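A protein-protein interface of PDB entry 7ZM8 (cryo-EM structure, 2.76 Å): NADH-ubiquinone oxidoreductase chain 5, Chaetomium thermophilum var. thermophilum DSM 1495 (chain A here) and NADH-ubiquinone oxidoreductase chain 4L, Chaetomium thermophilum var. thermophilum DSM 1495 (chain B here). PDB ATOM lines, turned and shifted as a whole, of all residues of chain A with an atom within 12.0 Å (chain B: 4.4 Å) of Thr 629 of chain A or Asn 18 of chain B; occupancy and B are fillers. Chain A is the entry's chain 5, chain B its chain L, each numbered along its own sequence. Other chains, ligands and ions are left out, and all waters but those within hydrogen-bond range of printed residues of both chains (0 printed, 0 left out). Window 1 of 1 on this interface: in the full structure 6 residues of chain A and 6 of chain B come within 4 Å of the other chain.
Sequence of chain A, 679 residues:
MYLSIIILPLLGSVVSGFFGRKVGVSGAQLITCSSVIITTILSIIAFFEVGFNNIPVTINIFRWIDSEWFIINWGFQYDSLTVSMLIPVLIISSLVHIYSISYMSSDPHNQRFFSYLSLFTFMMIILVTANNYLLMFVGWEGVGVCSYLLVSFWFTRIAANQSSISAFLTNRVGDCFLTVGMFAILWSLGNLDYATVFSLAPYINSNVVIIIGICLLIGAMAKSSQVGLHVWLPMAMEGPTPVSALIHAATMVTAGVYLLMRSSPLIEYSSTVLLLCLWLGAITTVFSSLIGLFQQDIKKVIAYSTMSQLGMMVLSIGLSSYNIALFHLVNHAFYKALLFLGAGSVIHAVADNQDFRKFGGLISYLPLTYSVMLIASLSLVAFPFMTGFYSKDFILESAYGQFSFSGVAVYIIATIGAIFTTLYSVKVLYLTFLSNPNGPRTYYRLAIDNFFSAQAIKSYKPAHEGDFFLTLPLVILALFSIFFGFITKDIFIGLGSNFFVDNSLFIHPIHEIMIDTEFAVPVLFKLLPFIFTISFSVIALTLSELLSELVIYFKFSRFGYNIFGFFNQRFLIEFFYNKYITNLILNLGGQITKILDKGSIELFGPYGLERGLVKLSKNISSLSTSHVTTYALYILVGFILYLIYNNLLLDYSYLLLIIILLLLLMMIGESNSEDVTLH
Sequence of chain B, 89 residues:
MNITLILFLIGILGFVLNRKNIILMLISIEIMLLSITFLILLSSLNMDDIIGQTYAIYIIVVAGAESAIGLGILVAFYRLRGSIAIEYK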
ATOM      1  N   LEU A 623      -9.981  34.594  10.801  1.00  0.00           N
ATOM      2  CA  LEU A 623     -11.260  34.014  11.187  1.00  0.00           C
ATOM      3  C   LEU A 623     -12.390  34.507  10.296  1.00  0.00           C
ATOM      4  O   LEU A 623     -13.481  33.930  10.307  1.00  0.00           O
ATOM      5  CB  LEU A 623     -11.569  34.341  12.646  1.00  0.00           C
ATOM      6  CG  LEU A 623     -10.700  33.684  13.714  1.00  0.00           C
ATOM      7  CD1 LEU A 623     -10.827  34.430  15.029  1.00  0.00           C
ATOM      8  CD2 LEU A 623     -11.083  32.231  13.885  1.00  0.00           C
ATOM      9  N   SER A 624     -12.155  35.566   9.527  1.00  0.00           N
ATOM     10  CA  SER A 624     -13.204  36.228   8.755  1.00  0.00           C
ATOM     11  C   SER A 624     -13.150  35.737   7.317  1.00  0.00           C
ATOM     12  O   SER A 624     -12.435  36.297   6.485  1.00  0.00           O
ATOM     13  CB  SER A 624     -13.039  37.739   8.824  1.00  0.00           C
ATOM     14  OG  SER A 624     -11.844  38.138   8.177  1.00  0.00           O
ATOM     15  N   THR A 625     -13.927  34.702   7.012  1.00  0.00           N
ATOM     16  CA  THR A 625     -13.895  34.066   5.706  1.00  0.00           C
ATOM     17  C   THR A 625     -15.066  34.468   4.820  1.00  0.00           C
ATOM     18  O   THR A 625     -15.221  33.913   3.730  1.00  0.00           O
ATOM     19  CB  THR A 625     -13.852  32.549   5.870  1.00  0.00           C
ATOM     20  OG1 THR A 625     -15.031  32.109   6.551  1.00  0.00           O
ATOM     21  CG2 THR A 625     -12.632  32.144   6.677  1.00  0.00           C
ATOM     22  N   SER A 626     -15.876  35.431   5.260  1.00  0.00           N
ATOM     23  CA  SER A 626     -17.053  35.900   4.528  1.00  0.00           C
ATOM     24  C   SER A 626     -18.002  34.758   4.182  1.00  0.00           C
ATOM     25  O   SER A 626     -18.623  34.755   3.117  1.00  0.00           O
ATOM     26  CB  SER A 626     -16.661  36.667   3.264  1.00  0.00           C
ATOM     27  OG  SER A 626     -16.511  35.793   2.162  1.00  0.00           O
ATOM     28  N   HIS A 627     -18.119  33.774   5.068  1.00  0.00           N
ATOM     29  CA  HIS A 627     -19.138  32.744   4.954  1.00  0.00           C
ATOM     30  C   HIS A 627     -20.239  33.061   5.950  1.00  0.00           C
ATOM     31  O   HIS A 627     -19.978  33.185   7.149  1.00  0.00           O
ATOM     32  CB  HIS A 627     -18.574  31.351   5.212  1.00  0.00           C
ATOM     33  CG  HIS A 627     -17.444  30.982   4.308  1.00  0.00           C
ATOM     34  ND1 HIS A 627     -16.233  30.528   4.780  1.00  0.00           N
ATOM     35  CD2 HIS A 627     -17.339  31.006   2.960  1.00  0.00           C
ATOM     36  CE1 HIS A 627     -15.430  30.286   3.761  1.00  0.00           C
ATOM     37  NE2 HIS A 627     -16.075  30.571   2.645  1.00  0.00           N
ATOM     38  N   VAL A 628     -21.463  33.210   5.451  1.00  0.00           N
ATOM     39  CA  VAL A 628     -22.586  33.493   6.333  1.00  0.00           C
ATOM     40  C   VAL A 628     -22.839  32.334   7.281  1.00  0.00           C
ATOM     41  O   VAL A 628     -23.256  32.540   8.423  1.00  0.00           O
ATOM     42  CB  VAL A 628     -23.832  33.855   5.502  1.00  0.00           C
ATOM     43  CG1 VAL A 628     -23.594  35.144   4.776  1.00  0.00           C
ATOM     44  CG2 VAL A 628     -24.080  32.786   4.478  1.00  0.00           C
ATOM     45  N   THR A 629     -22.605  31.104   6.828  1.00  0.00           N
ATOM     46  CA  THR A 629     -22.787  29.957   7.706  1.00  0.00           C
ATOM     47  C   THR A 629     -21.819  29.994   8.879  1.00  0.00           C
ATOM     48  O   THR A 629     -22.207  29.707  10.015  1.00  0.00           O
ATOM     49  CB  THR A 629     -22.640  28.658   6.911  1.00  0.00           C
ATOM     50  OG1 THR A 629     -21.347  28.604   6.299  1.00  0.00           O
ATOM     51  CG2 THR A 629     -23.716  28.546   5.852  1.00  0.00           C
ATOM     52  N   THR A 630     -20.557  30.350   8.634  1.00  0.00           N
ATOM     53  CA  THR A 630     -19.602  30.399   9.735  1.00  0.00           C
ATOM     54  C   THR A 630     -19.780  31.646  10.595  1.00  0.00           C
ATOM     55  O   THR A 630     -19.471  31.613  11.791  1.00  0.00           O
ATOM     56  CB  THR A 630     -18.163  30.300   9.216  1.00  0.00           C
ATOM     57  OG1 THR A 630     -17.292  30.001  10.309  1.00  0.00           O
ATOM     58  CG2 THR A 630     -17.702  31.596   8.622  1.00  0.00           C
ATOM     59  N   TYR A 631     -20.271  32.746  10.022  1.00  0.00           N
ATOM     60  CA  TYR A 631     -20.532  33.934  10.827  1.00  0.00           C
ATOM     61  C   TYR A 631     -21.714  33.712  11.756  1.00  0.00           C
ATOM     62  O   TYR A 631     -21.723  34.203  12.888  1.00  0.00           O
ATOM     63  CB  TYR A 631     -20.789  35.141   9.927  1.00  0.00           C
ATOM     64  CG  TYR A 631     -19.550  35.734   9.301  1.00  0.00           C
ATOM     65  CD1 TYR A 631     -18.287  35.302   9.665  1.00  0.00           C
ATOM     66  CD2 TYR A 631     -19.650  36.726   8.341  1.00  0.00           C
ATOM     67  CE1 TYR A 631     -17.157  35.844   9.088  1.00  0.00           C
ATOM     68  CE2 TYR A 631     -18.528  37.269   7.761  1.00  0.00           C
ATOM     69  CZ  TYR A 631     -17.285  36.826   8.139  1.00  0.00           C
ATOM     70  OH  TYR A 631     -16.172  37.372   7.554  1.00  0.00           O
ATOM     71  N   ALA A 632     -22.725  32.983  11.285  1.00  0.00           N
ATOM     72  CA  ALA A 632     -23.879  32.675  12.117  1.00  0.00           C
ATOM     73  C   ALA A 632     -23.482  31.836  13.320  1.00  0.00           C
ATOM     74  O   ALA A 632     -23.994  32.038  14.425  1.00  0.00           O
ATOM     75  CB  ALA A 632     -24.927  31.949  11.286  1.00  0.00           C
ATOM     76  N   LEU A 633     -22.568  30.888  13.120  1.00  0.00           N
ATOM     77  CA  LEU A 633     -22.079  30.078  14.226  1.00  0.00           C
ATOM     78  C   LEU A 633     -21.373  30.940  15.261  1.00  0.00           C
ATOM     79  O   LEU A 633     -21.489  30.696  16.467  1.00  0.00           O
ATOM     80  CB  LEU A 633     -21.147  28.996  13.687  1.00  0.00           C
ATOM     81  CG  LEU A 633     -20.922  27.757  14.544  1.00  0.00           C
ATOM     82  CD1 LEU A 633     -22.240  27.055  14.799  1.00  0.00           C
ATOM     83  CD2 LEU A 633     -19.941  26.820  13.861  1.00  0.00           C
ATOM     84  N   TYR A 634     -20.643  31.960  14.809  1.00  0.00           N
ATOM     85  CA  TYR A 634     -19.946  32.853  15.728  1.00  0.00           C
ATOM     86  C   TYR A 634     -20.923  33.634  16.596  1.00  0.00           C
ATOM     87  O   TYR A 634     -20.687  33.815  17.795  1.00  0.00           O
ATOM     88  CB  TYR A 634     -19.052  33.816  14.949  1.00  0.00           C
ATOM     89  CG  TYR A 634     -17.856  33.178  14.292  1.00  0.00           C
ATOM     90  CD1 TYR A 634     -17.449  31.899  14.635  1.00  0.00           C
ATOM     91  CD2 TYR A 634     -17.131  33.857  13.327  1.00  0.00           C
ATOM     92  CE1 TYR A 634     -16.354  31.316  14.037  1.00  0.00           C
ATOM     93  CE2 TYR A 634     -16.031  33.282  12.724  1.00  0.00           C
ATOM     94  CZ  TYR A 634     -15.648  32.011  13.084  1.00  0.00           C
ATOM     95  OH  TYR A 634     -14.561  31.425  12.488  1.00  0.00           O
ATOM     96  N   ILE A 635     -22.018  34.112  16.007  1.00  0.00           N
ATOM     97  CA  ILE A 635     -23.008  34.867  16.772  1.00  0.00           C
ATOM     98  C   ILE A 635     -23.624  33.999  17.858  1.00  0.00           C
ATOM     99  O   ILE A 635     -23.820  34.449  18.992  1.00  0.00           O
ATOM    100  CB  ILE A 635     -24.079  35.451  15.836  1.00  0.00           C
ATOM    101  CG1 ILE A 635     -23.447  36.446  14.869  1.00  0.00           C
ATOM    102  CG2 ILE A 635     -25.186  36.107  16.635  1.00  0.00           C
ATOM    103  CD1 ILE A 635     -24.361  36.874  13.757  1.00  0.00           C
ATOM    104  N   LEU A 636     -23.949  32.746  17.530  1.00  0.00           N
ATOM    105  CA  LEU A 636     -24.446  31.830  18.550  1.00  0.00           C
ATOM    106  C   LEU A 636     -23.406  31.592  19.631  1.00  0.00           C
ATOM    107  O   LEU A 636     -23.738  31.565  20.820  1.00  0.00           O
ATOM    108  CB  LEU A 636     -24.862  30.504  17.918  1.00  0.00           C
ATOM    109  CG  LEU A 636     -26.314  30.334  17.483  1.00  0.00           C
ATOM    110  CD1 LEU A 636     -27.170  30.153  18.720  1.00  0.00           C
ATOM    111  CD2 LEU A 636     -26.814  31.501  16.640  1.00  0.00           C
ATOM    112  N   VAL A 637     -22.145  31.416  19.240  1.00  0.00           N
ATOM    113  CA  VAL A 637     -21.089  31.201  20.221  1.00  0.00           C
ATOM    114  C   VAL A 637     -20.980  32.401  21.146  1.00  0.00           C
ATOM    115  O   VAL A 637     -21.029  32.267  22.373  1.00  0.00           O
ATOM    116  CB  VAL A 637     -19.755  30.911  19.512  1.00  0.00           C
ATOM    117  CG1 VAL A 637     -18.596  31.019  20.490  1.00  0.00           C
ATOM    118  CG2 VAL A 637     -19.790  29.542  18.871  1.00  0.00           C
ATOM    119  N   GLY A 638     -20.880  33.599  20.572  1.00  0.00           N
ATOM    120  CA  GLY A 638     -20.822  34.804  21.378  1.00  0.00           C
ATOM    121  C   GLY A 638     -22.086  35.067  22.158  1.00  0.00           C
ATOM    122  O   GLY A 638     -22.045  35.777  23.167  1.00  0.00           O
ATOM    123  N   GLY B  14     -30.687  24.563  13.504  1.00  0.00           N
ATOM    124  CA  GLY B  14     -30.566  24.697  12.066  1.00  0.00           C
ATOM    125  C   GLY B  14     -29.349  25.509  11.669  1.00  0.00           C
ATOM    126  O   GLY B  14     -28.725  25.247  10.642  1.00  0.00           O
ATOM    127  N   PHE B  15     -29.004  26.513  12.475  1.00  0.00           N
ATOM    128  CA  PHE B  15     -27.777  27.268  12.263  1.00  0.00           C
ATOM    129  C   PHE B  15     -26.551  26.509  12.753  1.00  0.00           C
ATOM    130  O   PHE B  15     -25.447  26.724  12.246  1.00  0.00           O
ATOM    131  CB  PHE B  15     -27.876  28.621  12.967  1.00  0.00           C
ATOM    132  CG  PHE B  15     -28.605  29.664  12.172  1.00  0.00           C
ATOM    133  CD1 PHE B  15     -29.980  29.702  12.155  1.00  0.00           C
ATOM    134  CD2 PHE B  15     -27.914  30.591  11.426  1.00  0.00           C
ATOM    135  CE1 PHE B  15     -30.642  30.654  11.412  1.00  0.00           C
ATOM    136  CE2 PHE B  15     -28.575  31.542  10.684  1.00  0.00           C
ATOM    137  CZ  PHE B  15     -29.937  31.573  10.680  1.00  0.00           C
ATOM    138  N   VAL B  16     -26.723  25.631  13.741  1.00  0.00           N
ATOM    139  CA  VAL B  16     -25.602  24.848  14.251  1.00  0.00           C
ATOM    140  C   VAL B  16     -25.138  23.828  13.220  1.00  0.00           C
ATOM    141  O   VAL B  16     -23.942  23.533  13.114  1.00  0.00           O
ATOM    142  CB  VAL B  16     -25.991  24.172  15.578  1.00  0.00           C
ATOM    143  CG1 VAL B  16     -24.837  23.340  16.113  1.00  0.00           C
ATOM    144  CG2 VAL B  16     -26.414  25.215  16.598  1.00  0.00           C
ATOM    145  N   LEU B  17     -26.069  23.272  12.448  1.00  0.00           N
ATOM    146  CA  LEU B  17     -25.783  22.152  11.564  1.00  0.00           C
ATOM    147  C   LEU B  17     -25.683  22.559  10.099  1.00  0.00           C
ATOM    148  O   LEU B  17     -25.855  21.708   9.220  1.00  0.00           O
ATOM    149  CB  LEU B  17     -26.853  21.072  11.721  1.00  0.00           C
ATOM    150  CG  LEU B  17     -27.041  20.445  13.098  1.00  0.00           C
ATOM    151  CD1 LEU B  17     -28.134  19.398  13.046  1.00  0.00           C
ATOM    152  CD2 LEU B  17     -25.747  19.834  13.567  1.00  0.00           C
ATOM    153  N   ASN B  18     -25.414  23.828   9.809  1.00  0.00           N
ATOM    154  CA  ASN B  18     -25.498  24.332   8.443  1.00  0.00           C
ATOM    155  C   ASN B  18     -24.173  24.946   8.018  1.00  0.00           C
ATOM    156  O   ASN B  18     -23.791  26.011   8.508  1.00  0.00           O
ATOM    157  CB  ASN B  18     -26.621  25.351   8.312  1.00  0.00           C
ATOM    158  CG  ASN B  18     -27.105  25.483   6.897  1.00  0.00           C
ATOM    159  OD1 ASN B  18     -26.752  24.680   6.039  1.00  0.00           O
ATOM    160  ND2 ASN B  18     -27.905  26.502   6.635  1.00  0.00           N
ATOM    161  N   ARG B  19     -23.493  24.289   7.078  1.00  0.00           N
ATOM    162  CA  ARG B  19     -22.312  24.846   6.444  1.00  0.00           C
ATOM    163  C   ARG B  19     -22.535  25.264   5.001  1.00  0.00           C
ATOM    164  O   ARG B  19     -21.718  26.017   4.464  1.00  0.00           O
ATOM    165  CB  ARG B  19     -21.159  23.833   6.476  1.00  0.00           C
ATOM    166  CG  ARG B  19     -20.735  23.398   7.852  1.00  0.00           C
ATOM    167  CD  ARG B  19     -19.802  24.407   8.499  1.00  0.00           C
ATOM    168  NE  ARG B  19     -20.519  25.512   9.132  1.00  0.00           N
ATOM    169  CZ  ARG B  19     -21.275  25.396  10.218  1.00  0.00           C
ATOM    170  NH1 ARG B  19     -21.882  26.462  10.716  1.00  0.00           N
ATOM    171  NH2 ARG B  19     -21.423  24.220  10.809  1.00  0.00           N
ATOM    172  N   LYS B  20     -23.604  24.798   4.357  1.00  0.00           N
ATOM    173  CA  LYS B  20     -23.746  25.022   2.926  1.00  0.00           C
ATOM    174  C   LYS B  20     -25.078  25.653   2.534  1.00  0.00           C
ATOM    175  O   LYS B  20     -25.120  26.489   1.627  1.00  0.00           O
ATOM    176  CB  LYS B  20     -23.565  23.701   2.181  1.00  0.00           C
ATOM    177  CG  LYS B  20     -22.407  22.851   2.670  1.00  0.00           C
ATOM    178  CD  LYS B  20     -21.114  23.231   1.977  1.00  0.00           C
ATOM    179  CE  LYS B  20     -20.140  22.065   1.949  1.00  0.00           C
ATOM    180  NZ  LYS B  20     -20.571  21.006   0.994  1.00  0.00           N
ATOM    181  N   ASN B  21     -26.167  25.258   3.190  1.00  0.00           N
ATOM    182  CA  ASN B  21     -27.494  25.773   2.862  1.00  0.00           C
ATOM    183  C   ASN B  21     -27.629  27.204   3.357  1.00  0.00           C
ATOM    184  O   ASN B  21     -27.662  27.446   4.565  1.00  0.00           O
ATOM    185  CB  ASN B  21     -28.589  24.924   3.497  1.00  0.00           C
ATOM    186  CG  ASN B  21     -28.780  23.607   2.832  1.00  0.00           C
ATOM    187  OD1 ASN B  21     -28.809  23.519   1.614  1.00  0.00           O
ATOM    188  ND2 ASN B  21     -28.904  22.560   3.628  1.00  0.00           N
ATOM    189  N   LEU B  24     -31.538  27.004   4.073  1.00  0.00           N
ATOM    190  CA  LEU B  24     -31.922  26.491   5.380  1.00  0.00           C
ATOM    191  C   LEU B  24     -31.750  27.533   6.480  1.00  0.00           C
ATOM    192  O   LEU B  24     -32.382  27.414   7.533  1.00  0.00           O
ATOM    193  CB  LEU B  24     -31.124  25.227   5.691  1.00  0.00           C
ATOM    194  CG  LEU B  24     -31.373  24.391   6.943  1.00  0.00           C
ATOM    195  CD1 LEU B  24     -32.795  23.855   6.971  1.00  0.00           C
ATOM    196  CD2 LEU B  24     -30.368  23.256   6.994  1.00  0.00           C
ATOM    197  N   MET B  25     -30.918  28.562   6.267  1.00  0.00           N
ATOM    198  CA  MET B  25     -30.896  29.667   7.224  1.00  0.00           C
ATOM    199  C   MET B  25     -32.133  30.545   7.099  1.00  0.00           C
ATOM    200  O   MET B  25     -32.584  31.124   8.089  1.00  0.00           O
ATOM    201  CB  MET B  25     -29.637  30.524   7.089  1.00  0.00           C
ATOM    202  CG  MET B  25     -28.349  29.841   7.468  1.00  0.00           C
ATOM    203  SD  MET B  25     -26.979  30.996   7.342  1.00  0.00           S
ATOM    204  CE  MET B  25     -26.819  31.094   5.580  1.00  0.00           C
ATOM    205  N   ILE B  86     -22.377  27.626  -1.072  1.00  0.00           N
ATOM    206  CA  ILE B  86     -21.142  28.158  -0.512  1.00  0.00           C
ATOM    207  C   ILE B  86     -19.996  27.182  -0.759  1.00  0.00           C
ATOM    208  O   ILE B  86     -20.075  25.986  -0.456  1.00  0.00           O
ATOM    209  CB  ILE B  86     -21.297  28.466   0.987  1.00  0.00           C
ATOM    210  CG1 ILE B  86     -22.279  29.615   1.195  1.00  0.00           C
ATOM    211  CG2 ILE B  86     -19.959  28.807   1.613  1.00  0.00           C
ATOM    212  CD1 ILE B  86     -22.685  29.810   2.629  1.00  0.00           C
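The backbone carbonyl oxygen of Arg 19 of chain B is in hydrogen-bond range of the side-chain hydroxyl of Thr 629 of chain A, at 3.2 Å.
OD1 of Asn 18 of chain B sits at hydrogen-bond distance from N of Asn 21 of chain B, 3.0 Å away. The side-chain hydroxyl (OG1) of Thr 625 of chain A lies within hydrogen-bond range of a ring nitrogen (ND1) of His 627 of chain A (2.7 Å). The backbone carbonyl oxygen (O) of Val 16 of chain B sits at hydrogen-bond distance from the guanidinium group (NH2) of Arg 19 of chain B, at 3.5 Å.
CG2 of Ile 86 of chain B touches CD2 of His 627 of chain A, at 3.7 Å. Val 628 of chain A touches Met 25 of chain B. Ile 86 of chain B touches Val 628 of chain A. Asn 18 of chain B touches Thr 629 of chain A. Thr 629 of chain A touches Ile 86 of chain B. Ala 632 of chain A touches Phe 15 of chain B (CB to CD2, 3.3 Å). Leu 633 of chain A touches Arg 19 of chain B.
Thr 629 of chain A touches three residues of chain B. Of chain A, only Thr 629 comes within 4 Å of Asn 18 of chain B. No residue of chain A comes within 4 Å of Gly 14 of chain B. No residue of chain A comes within 4 Å of Val 16 of chain B. No residue of chain A comes within 4 Å of Leu 17 of chain B. Arg 19 of chain B touches just these residues of chain A: Thr 629 and Leu 633. Ile 86 of chain B touches three residues of chain A. Of the printed residues of chain B, Ala 632 of chain A touches Phe 15. Of the printed residues of chain B, His 627 of chain A touches Ile 86 (3.7 Å). Printed residues of chain B within 4 Å of Val 628 of chain A: Met 25 and Ile 86. Of the printed residues of chain B, Leu 633 of chain A touches Arg 19 (3.7 Å). Tyr 634 of chain A touches none of the printed residues of chain B. The nearest printed residue of chain B that does not touch Thr 629 of chain A is Met 25 of chain B (4.02 Å).
Of the 11 printed residues of chain B, 5 touch a printed residue of chain A. Among the printed residues, 8 pairs touch across the chains. Among the printed residues, no Asp or Glu carboxylate lies within 4 Å of a Lys or Arg side-chain nitrogen of the other chain.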
